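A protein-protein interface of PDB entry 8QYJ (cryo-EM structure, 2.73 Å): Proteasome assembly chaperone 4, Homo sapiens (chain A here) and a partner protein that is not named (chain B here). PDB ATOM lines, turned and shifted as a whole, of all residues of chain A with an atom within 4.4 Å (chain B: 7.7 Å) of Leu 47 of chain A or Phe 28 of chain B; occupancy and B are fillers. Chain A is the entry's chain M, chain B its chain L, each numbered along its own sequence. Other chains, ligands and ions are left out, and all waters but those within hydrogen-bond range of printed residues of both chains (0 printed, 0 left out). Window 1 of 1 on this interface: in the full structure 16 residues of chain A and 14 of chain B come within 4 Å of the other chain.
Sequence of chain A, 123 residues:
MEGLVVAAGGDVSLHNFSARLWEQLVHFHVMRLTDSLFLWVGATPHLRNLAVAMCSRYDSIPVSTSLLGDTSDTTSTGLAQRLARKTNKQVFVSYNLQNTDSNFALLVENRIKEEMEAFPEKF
Of the 8 printed residues of chain A, 4 touch a printed residue of chain B.
Hydrophobic or aromatic side chains of chain A within 4 Å of the printed part of chain B: Trp 40, Pro 45, His 46 and Leu 47.
Hydrophobic or aromatic side chains of chain B that line the printed part of chain A: Leu 6, Phe 28 and His 31.
Among the printed residues, no Asp or Glu carboxylate lies within 4 Å of a Lys or Arg side-chain nitrogen of the other chain.
The backbone NH (N) of Ser 29 of chain B is in hydrogen-bond range of the backbone carbonyl oxygen (O) of Pro 45 of chain A (3.0 Å).
The side-chain hydroxyl of Ser 30 of chain B sits at hydrogen-bond distance from the backbone NH of Leu 47 of chain A.
Of the printed residues of chain B, Trp 40 of chain A touches Phe 28 (3.7 Å).
Printed residues of chain B within 4 Å of Pro 45 of chain A: Leu 6 and Ser 29.
Leu 47 of chain A touches three residues of chain B.
Cys 25 of chain B touches none of the printed residues of chain A.
Of chain A, only Trp 40 (3.7 Å) and Leu 47 (3.7 Å) come within 4 Å of Phe 28 of chain B.
Of the printed residues of chain A, Ser 29 of chain B touches Pro 45 and His 46.
Of the printed residues of chain A, His 31 of chain B touches Leu 47.
The nearest printed residue of chain A that does not touch His 31 of chain B is Arg 48 of chain A (5.7 Å).
Among the printed residues, pairs that only touch across the chains: Trp 40 of chain A with Phe 28 of chain B, Pro 45 of chain A with Leu 6 of chain B, His 46 of chain A with Ser 29 of chain B, His 46 of chain A with Ser 30 of chain B, Leu 47 of chain A with Phe 28 of chain B and Leu 47 of chain A with His 31 of chain B.
The backbone carbonyl oxygen (O) of Phe 28 of chain B is in hydrogen-bond range of the guanidinium group (NH1) of Arg 93 of chain B (3.0 Å).
The backbone carbonyl oxygen of His 46 of chain A sits at hydrogen-bond distance from the indole nitrogen of Trp 40 of chain A (2.9 Å).
The indole nitrogen (NE1) of Trp 40 of chain A lies close to the side-chain amide nitrogen (ND2) of Asn 96 of chain A (3.0 Å).
The backbone carbonyl oxygen of His 46 of chain A sits at hydrogen-bond distance from the side-chain amide nitrogen of Asn 96 of chain A (3.4 Å).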
ATOM      1  N   TRP A  40      -9.864  16.957  23.959  1.00  0.00           N
ATOM      2  CA  TRP A  40     -10.417  16.258  22.806  1.00  0.00           C
ATOM      3  C   TRP A  40      -9.731  16.757  21.543  1.00  0.00           C
ATOM      4  O   TRP A  40      -9.644  17.967  21.318  1.00  0.00           O
ATOM      5  CB  TRP A  40     -11.931  16.466  22.709  1.00  0.00           C
ATOM      6  CG  TRP A  40     -12.548  15.852  21.489  1.00  0.00           C
ATOM      7  CD1 TRP A  40     -13.046  14.590  21.371  1.00  0.00           C
ATOM      8  CD2 TRP A  40     -12.738  16.478  20.214  1.00  0.00           C
ATOM      9  NE1 TRP A  40     -13.531  14.387  20.103  1.00  0.00           N
ATOM     10  CE2 TRP A  40     -13.354  15.532  19.373  1.00  0.00           C
ATOM     11  CE3 TRP A  40     -12.445  17.745  19.703  1.00  0.00           C
ATOM     12  CZ2 TRP A  40     -13.682  15.813  18.050  1.00  0.00           C
ATOM     13  CZ3 TRP A  40     -12.771  18.021  18.390  1.00  0.00           C
ATOM     14  CH2 TRP A  40     -13.383  17.060  17.578  1.00  0.00           C
ATOM     15  N   PRO A  45     -16.514  15.807  14.299  1.00  0.00           N
ATOM     16  CA  PRO A  45     -17.103  15.757  15.645  1.00  0.00           C
ATOM     17  C   PRO A  45     -17.474  14.347  16.076  1.00  0.00           C
ATOM     18  O   PRO A  45     -18.657  14.016  16.184  1.00  0.00           O
ATOM     19  CB  PRO A  45     -18.347  16.648  15.524  1.00  0.00           C
ATOM     20  CG  PRO A  45     -18.196  17.387  14.229  1.00  0.00           C
ATOM     21  CD  PRO A  45     -17.390  16.502  13.344  1.00  0.00           C
ATOM     22  N   HIS A  46     -16.472  13.511  16.337  1.00  0.00           N
ATOM     23  CA  HIS A  46     -16.691  12.145  16.783  1.00  0.00           C
ATOM     24  C   HIS A  46     -15.907  11.893  18.061  1.00  0.00           C
ATOM     25  O   HIS A  46     -14.855  12.494  18.293  1.00  0.00           O
ATOM     26  CB  HIS A  46     -16.279  11.125  15.713  1.00  0.00           C
ATOM     27  CG  HIS A  46     -17.288  10.951  14.622  1.00  0.00           C
ATOM     28  ND1 HIS A  46     -17.399  11.827  13.564  1.00  0.00           N
ATOM     29  CD2 HIS A  46     -18.231  10.000  14.423  1.00  0.00           C
ATOM     30  CE1 HIS A  46     -18.367  11.424  12.761  1.00  0.00           C
ATOM     31  NE2 HIS A  46     -18.889  10.318  13.260  1.00  0.00           N
ATOM     32  N   LEU A  47     -16.435  10.996  18.890  1.00  0.00           N
ATOM     33  CA  LEU A  47     -15.799  10.598  20.145  1.00  0.00           C
ATOM     34  C   LEU A  47     -15.834   9.075  20.212  1.00  0.00           C
ATOM     35  O   LEU A  47     -16.884   8.484  20.479  1.00  0.00           O
ATOM     36  CB  LEU A  47     -16.500  11.229  21.345  1.00  0.00           C
ATOM     37  CG  LEU A  47     -15.727  11.303  22.663  1.00  0.00           C
ATOM     38  CD1 LEU A  47     -16.187  12.495  23.481  1.00  0.00           C
ATOM     39  CD2 LEU A  47     -15.885  10.022  23.466  1.00  0.00           C
ATOM     40  N   ARG A  48     -14.687   8.440  19.969  1.00  0.00           N
ATOM     41  CA  ARG A  48     -14.591   6.990  20.032  1.00  0.00           C
ATOM     42  C   ARG A  48     -13.449   6.492  20.905  1.00  0.00           C
ATOM     43  O   ARG A  48     -13.313   5.277  21.075  1.00  0.00           O
ATOM     44  CB  ARG A  48     -14.440   6.397  18.623  1.00  0.00           C
ATOM     45  CG  ARG A  48     -13.653   7.264  17.661  1.00  0.00           C
ATOM     46  CD  ARG A  48     -13.610   6.648  16.273  1.00  0.00           C
ATOM     47  NE  ARG A  48     -12.840   7.460  15.340  1.00  0.00           N
ATOM     48  CZ  ARG A  48     -11.532   7.351  15.153  1.00  0.00           C
ATOM     49  NH1 ARG A  48     -10.810   6.468  15.823  1.00  0.00           N
ATOM     50  NH2 ARG A  48     -10.933   8.147  14.273  1.00  0.00           N
ATOM     51  N   ASN A  49     -12.631   7.382  21.463  1.00  0.00           N
ATOM     52  CA  ASN A  49     -11.520   6.998  22.321  1.00  0.00           C
ATOM     53  C   ASN A  49     -11.534   7.846  23.584  1.00  0.00           C
ATOM     54  O   ASN A  49     -11.955   9.006  23.565  1.00  0.00           O
ATOM     55  CB  ASN A  49     -10.173   7.160  21.604  1.00  0.00           C
ATOM     56  CG  ASN A  49      -9.980   6.149  20.491  1.00  0.00           C
ATOM     57  OD1 ASN A  49     -10.002   4.942  20.723  1.00  0.00           O
ATOM     58  ND2 ASN A  49      -9.785   6.641  19.274  1.00  0.00           N
ATOM     59  N   SER A  94      -8.887  12.368  24.726  1.00  0.00           N
ATOM     60  CA  SER A  94      -9.656  11.706  23.676  1.00  0.00           C
ATOM     61  C   SER A  94      -9.011  12.047  22.337  1.00  0.00           C
ATOM     62  O   SER A  94      -9.271  13.112  21.768  1.00  0.00           O
ATOM     63  CB  SER A  94     -11.119  12.132  23.716  1.00  0.00           C
ATOM     64  OG  SER A  94     -11.902  11.345  22.838  1.00  0.00           O
ATOM     65  N   ASN A  96      -8.814  11.216  18.532  1.00  0.00           N
ATOM     66  CA  ASN A  96      -9.665  10.583  17.536  1.00  0.00           C
ATOM     67  C   ASN A  96      -9.117  10.664  16.119  1.00  0.00           C
ATOM     68  O   ASN A  96      -9.785  10.198  15.188  1.00  0.00           O
ATOM     69  CB  ASN A  96     -11.070  11.199  17.574  1.00  0.00           C
ATOM     70  CG  ASN A  96     -11.794  10.910  18.870  1.00  0.00           C
ATOM     71  OD1 ASN A  96     -12.269   9.799  19.094  1.00  0.00           O
ATOM     72  ND2 ASN A  96     -11.877  11.911  19.735  1.00  0.00           N
ATOM     73  N   LEU B   6     -16.011  23.628  16.342  1.00  0.00           N
ATOM     74  CA  LEU B   6     -16.641  22.423  15.820  1.00  0.00           C
ATOM     75  C   LEU B   6     -17.589  21.782  16.825  1.00  0.00           C
ATOM     76  O   LEU B   6     -18.498  21.051  16.420  1.00  0.00           O
ATOM     77  CB  LEU B   6     -15.574  21.414  15.395  1.00  0.00           C
ATOM     78  CG  LEU B   6     -15.983  20.386  14.340  1.00  0.00           C
ATOM     79  CD1 LEU B   6     -16.193  21.053  12.992  1.00  0.00           C
ATOM     80  CD2 LEU B   6     -14.944  19.284  14.238  1.00  0.00           C
ATOM     81  N   VAL B   7     -17.403  22.042  18.117  1.00  0.00           N
ATOM     82  CA  VAL B   7     -18.251  21.495  19.169  1.00  0.00           C
ATOM     83  C   VAL B   7     -18.873  22.654  19.937  1.00  0.00           C
ATOM     84  O   VAL B   7     -18.186  23.625  20.276  1.00  0.00           O
ATOM     85  CB  VAL B   7     -17.466  20.556  20.106  1.00  0.00           C
ATOM     86  CG1 VAL B   7     -17.011  19.320  19.348  1.00  0.00           C
ATOM     87  CG2 VAL B   7     -16.266  21.267  20.709  1.00  0.00           C
ATOM     88  N   ILE B   8     -20.177  22.561  20.188  1.00  0.00           N
ATOM     89  CA  ILE B   8     -20.937  23.617  20.846  1.00  0.00           C
ATOM     90  C   ILE B   8     -21.230  23.185  22.274  1.00  0.00           C
ATOM     91  O   ILE B   8     -21.671  22.053  22.509  1.00  0.00           O
ATOM     92  CB  ILE B   8     -22.238  23.920  20.083  1.00  0.00           C
ATOM     93  CG1 ILE B   8     -21.921  24.351  18.649  1.00  0.00           C
ATOM     94  CG2 ILE B   8     -23.042  24.996  20.796  1.00  0.00           C
ATOM     95  CD1 ILE B   8     -21.084  25.604  18.563  1.00  0.00           C
ATOM     96  N   CYS B  25     -22.883  21.066  29.359  1.00  0.00           N
ATOM     97  CA  CYS B  25     -23.352  20.192  28.291  1.00  0.00           C
ATOM     98  C   CYS B  25     -22.557  20.473  27.027  1.00  0.00           C
ATOM     99  O   CYS B  25     -22.414  21.632  26.625  1.00  0.00           O
ATOM    100  CB  CYS B  25     -24.849  20.389  28.030  1.00  0.00           C
ATOM    101  SG  CYS B  25     -25.929  19.808  29.357  1.00  0.00           S
ATOM    102  N   THR B  26     -22.043  19.414  26.402  1.00  0.00           N
ATOM    103  CA  THR B  26     -21.284  19.512  25.164  1.00  0.00           C
ATOM    104  C   THR B  26     -21.796  18.469  24.184  1.00  0.00           C
ATOM    105  O   THR B  26     -22.015  17.313  24.557  1.00  0.00           O
ATOM    106  CB  THR B  26     -19.780  19.314  25.410  1.00  0.00           C
ATOM    107  OG1 THR B  26     -19.312  20.299  26.339  1.00  0.00           O
ATOM    108  CG2 THR B  26     -19.001  19.446  24.111  1.00  0.00           C
ATOM    109  N   ALA B  27     -21.985  18.876  22.932  1.00  0.00           N
ATOM    110  CA  ALA B  27     -22.622  18.043  21.922  1.00  0.00           C
ATOM    111  C   ALA B  27     -21.609  17.583  20.884  1.00  0.00           C
ATOM    112  O   ALA B  27     -20.860  18.396  20.332  1.00  0.00           O
ATOM    113  CB  ALA B  27     -23.761  18.799  21.235  1.00  0.00           C
ATOM    114  N   PHE B  28     -21.592  16.279  20.624  1.00  0.00           N
ATOM    115  CA  PHE B  28     -20.868  15.682  19.513  1.00  0.00           C
ATOM    116  C   PHE B  28     -21.865  15.056  18.545  1.00  0.00           C
ATOM    117  O   PHE B  28     -23.072  15.023  18.797  1.00  0.00           O
ATOM    118  CB  PHE B  28     -19.867  14.630  20.008  1.00  0.00           C
ATOM    119  CG  PHE B  28     -18.804  15.178  20.917  1.00  0.00           C
ATOM    120  CD1 PHE B  28     -17.613  15.659  20.401  1.00  0.00           C
ATOM    121  CD2 PHE B  28     -18.992  15.207  22.288  1.00  0.00           C
ATOM    122  CE1 PHE B  28     -16.633  16.161  21.234  1.00  0.00           C
ATOM    123  CE2 PHE B  28     -18.015  15.710  23.126  1.00  0.00           C
ATOM    124  CZ  PHE B  28     -16.835  16.187  22.598  1.00  0.00           C
ATOM    125  N   SER B  29     -21.351  14.556  17.423  1.00  0.00           N
ATOM    126  CA  SER B  29     -22.214  13.900  16.449  1.00  0.00           C
ATOM    127  C   SER B  29     -22.535  12.460  16.821  1.00  0.00           C
ATOM    128  O   SER B  29     -23.383  11.843  16.167  1.00  0.00           O
ATOM    129  CB  SER B  29     -21.577  13.936  15.058  1.00  0.00           C
ATOM    130  OG  SER B  29     -20.393  13.159  15.019  1.00  0.00           O
ATOM    131  N   SER B  30     -21.883  11.912  17.846  1.00  0.00           N
ATOM    132  CA  SER B  30     -22.160  10.559  18.305  1.00  0.00           C
ATOM    133  C   SER B  30     -22.462  10.468  19.793  1.00  0.00           C
ATOM    134  O   SER B  30     -22.993   9.441  20.229  1.00  0.00           O
ATOM    135  CB  SER B  30     -20.981   9.629  17.984  1.00  0.00           C
ATOM    136  OG  SER B  30     -19.756  10.194  18.420  1.00  0.00           O
ATOM    137  N   HIS B  31     -22.149  11.495  20.579  1.00  0.00           N
ATOM    138  CA  HIS B  31     -22.366  11.475  22.016  1.00  0.00           C
ATOM    139  C   HIS B  31     -22.804  12.855  22.479  1.00  0.00           C
ATOM    140  O   HIS B  31     -22.573  13.863  21.808  1.00  0.00           O
ATOM    141  CB  HIS B  31     -21.101  11.062  22.783  1.00  0.00           C
ATOM    142  CG  HIS B  31     -20.732   9.621  22.624  1.00  0.00           C
ATOM    143  ND1 HIS B  31     -21.006   8.673  23.585  1.00  0.00           N
ATOM    144  CD2 HIS B  31     -20.094   8.969  21.624  1.00  0.00           C
ATOM    145  CE1 HIS B  31     -20.562   7.497  23.180  1.00  0.00           C
ATOM    146  NE2 HIS B  31     -20.004   7.650  21.992  1.00  0.00           N
ATOM    147  N   ILE B  32     -23.443  12.886  23.644  1.00  0.00           N
ATOM    148  CA  ILE B  32     -23.721  14.118  24.370  1.00  0.00           C
ATOM    149  C   ILE B  32     -23.046  14.009  25.728  1.00  0.00           C
ATOM    150  O   ILE B  32     -23.284  13.048  26.467  1.00  0.00           O
ATOM    151  CB  ILE B  32     -25.233  14.369  24.527  1.00  0.00           C
ATOM    152  CG1 ILE B  32     -25.918  14.409  23.160  1.00  0.00           C
ATOM    153  CG2 ILE B  32     -25.483  15.659  25.294  1.00  0.00           C
ATOM    154  CD1 ILE B  32     -25.786  15.736  22.448  1.00  0.00           C
ATOM    155  N   LEU B  33     -22.203  14.985  26.051  1.00  0.00           N
ATOM    156  CA  LEU B  33     -21.436  14.975  27.290  1.00  0.00           C
ATOM    157  C   LEU B  33     -22.116  15.885  28.304  1.00  0.00           C
ATOM    158  O   LEU B  33     -22.221  17.097  28.086  1.00  0.00           O
ATOM    159  CB  LEU B  33     -19.997  15.424  27.039  1.00  0.00           C
ATOM    160  CG  LEU B  33     -19.100  15.594  28.266  1.00  0.00           C
ATOM    161  CD1 LEU B  33     -18.967  14.284  29.021  1.00  0.00           C
ATOM    162  CD2 LEU B  33     -17.734  16.118  27.859  1.00  0.00           C
ATOM    163  N   ALA B  90     -32.391  13.925  21.475  1.00  0.00           N
ATOM    164  CA  ALA B  90     -31.240  14.183  20.622  1.00  0.00           C
ATOM    165  C   ALA B  90     -31.224  13.312  19.374  1.00  0.00           C
ATOM    166  O   ALA B  90     -30.260  13.366  18.606  1.00  0.00           O
ATOM    167  CB  ALA B  90     -29.945  13.988  21.410  1.00  0.00           C
ATOM    168  N   ARG B  93     -29.382   9.322  20.474  1.00  0.00           N
ATOM    169  CA  ARG B  93     -27.931   9.395  20.508  1.00  0.00           C
ATOM    170  C   ARG B  93     -27.421   8.989  21.885  1.00  0.00           C
ATOM    171  O   ARG B  93     -28.105   9.168  22.896  1.00  0.00           O
ATOM    172  CB  ARG B  93     -27.443  10.805  20.164  1.00  0.00           C
ATOM    173  CG  ARG B  93     -26.124  10.837  19.416  1.00  0.00           C
ATOM    174  CD  ARG B  93     -25.667  12.260  19.143  1.00  0.00           C
ATOM    175  NE  ARG B  93     -26.611  12.993  18.310  1.00  0.00           N
ATOM    176  CZ  ARG B  93     -26.782  14.308  18.348  1.00  0.00           C
ATOM    177  NH1 ARG B  93     -26.072  15.072  19.162  1.00  0.00           N
ATOM    178  NH2 ARG B  93     -27.682  14.869  17.548  1.00  0.00           N
ATOM    179  N   ALA B  94     -26.211   8.437  21.913  1.00  0.00           N
ATOM    180  CA  ALA B  94     -25.614   7.998  23.166  1.00  0.00           C
ATOM    181  C   ALA B  94     -25.271   9.193  24.049  1.00  0.00           C
ATOM    182  O   ALA B  94     -25.026  10.302  23.568  1.00  0.00           O
ATOM    183  CB  ALA B  94     -24.360   7.169  22.898  1.00  0.00           C
ATOM    184  N   LEU B  96     -22.873  10.384  27.469  1.00  0.00           N
ATOM    185  CA  LEU B  96     -21.774  10.135  28.395  1.00  0.00           C
ATOM    186  C   LEU B  96     -21.950  11.076  29.580  1.00  0.00           C
ATOM    187  O   LEU B  96     -21.865  12.298  29.425  1.00  0.00           O
ATOM    188  CB  LEU B  96     -20.425  10.347  27.711  1.00  0.00           C
ATOM    189  CG  LEU B  96     -19.173   9.920  28.479  1.00  0.00           C
ATOM    190  CD1 LEU B  96     -19.161   8.415  28.689  1.00  0.00           C
ATOM    191  CD2 LEU B  96     -17.923  10.370  27.746  1.00  0.00           C
ATOM    192  N   VAL B 121     -28.279  21.916  24.163  1.00  0.00           N
ATOM    193  CA  VAL B 121     -27.425  22.202  23.014  1.00  0.00           C
ATOM    194  C   VAL B 121     -27.783  21.261  21.872  1.00  0.00           C
ATOM    195  O   VAL B 121     -27.372  21.472  20.726  1.00  0.00           O
ATOM    196  CB  VAL B 121     -25.933  22.078  23.375  1.00  0.00           C
ATOM    197  CG1 VAL B 121     -25.566  23.053  24.478  1.00  0.00           C
ATOM    198  CG2 VAL B 121     -25.605  20.655  23.790  1.00  0.00           C
ATOM    199  N   TRP B 122     -28.544  20.214  22.175  1.00  0.00           N
ATOM    200  CA  TRP B 122     -28.940  19.237  21.168  1.00  0.00           C
ATOM    201  C   TRP B 122     -30.114  19.744  20.339  1.00  0.00           C
ATOM    202  O   TRP B 122     -30.382  19.244  19.246  1.00  0.00           O
ATOM    203  CB  TRP B 122     -29.303  17.902  21.824  1.00  0.00           C
ATOM    204  CG  TRP B 122     -30.302  18.028  22.932  1.00  0.00           C
ATOM    205  CD1 TRP B 122     -31.649  17.840  22.845  1.00  0.00           C
ATOM    206  CD2 TRP B 122     -30.031  18.359  24.298  1.00  0.00           C
ATOM    207  NE1 TRP B 122     -32.235  18.042  24.070  1.00  0.00           N
ATOM    208  CE2 TRP B 122     -31.263  18.361  24.980  1.00  0.00           C
ATOM    209  CE3 TRP B 122     -28.866  18.658  25.012  1.00  0.00           C
ATOM    210  CZ2 TRP B 122     -31.364  18.647  26.338  1.00  0.00           C
ATOM    211  CZ3 TRP B 122     -28.969  18.943  26.359  1.00  0.00           C
ATOM    212  CH2 TRP B 122     -30.208  18.936  27.009  1.00  0.00           C
ATOM    213  OXT TRP B 122     -30.825  20.663  20.742  1.00  0.00           O
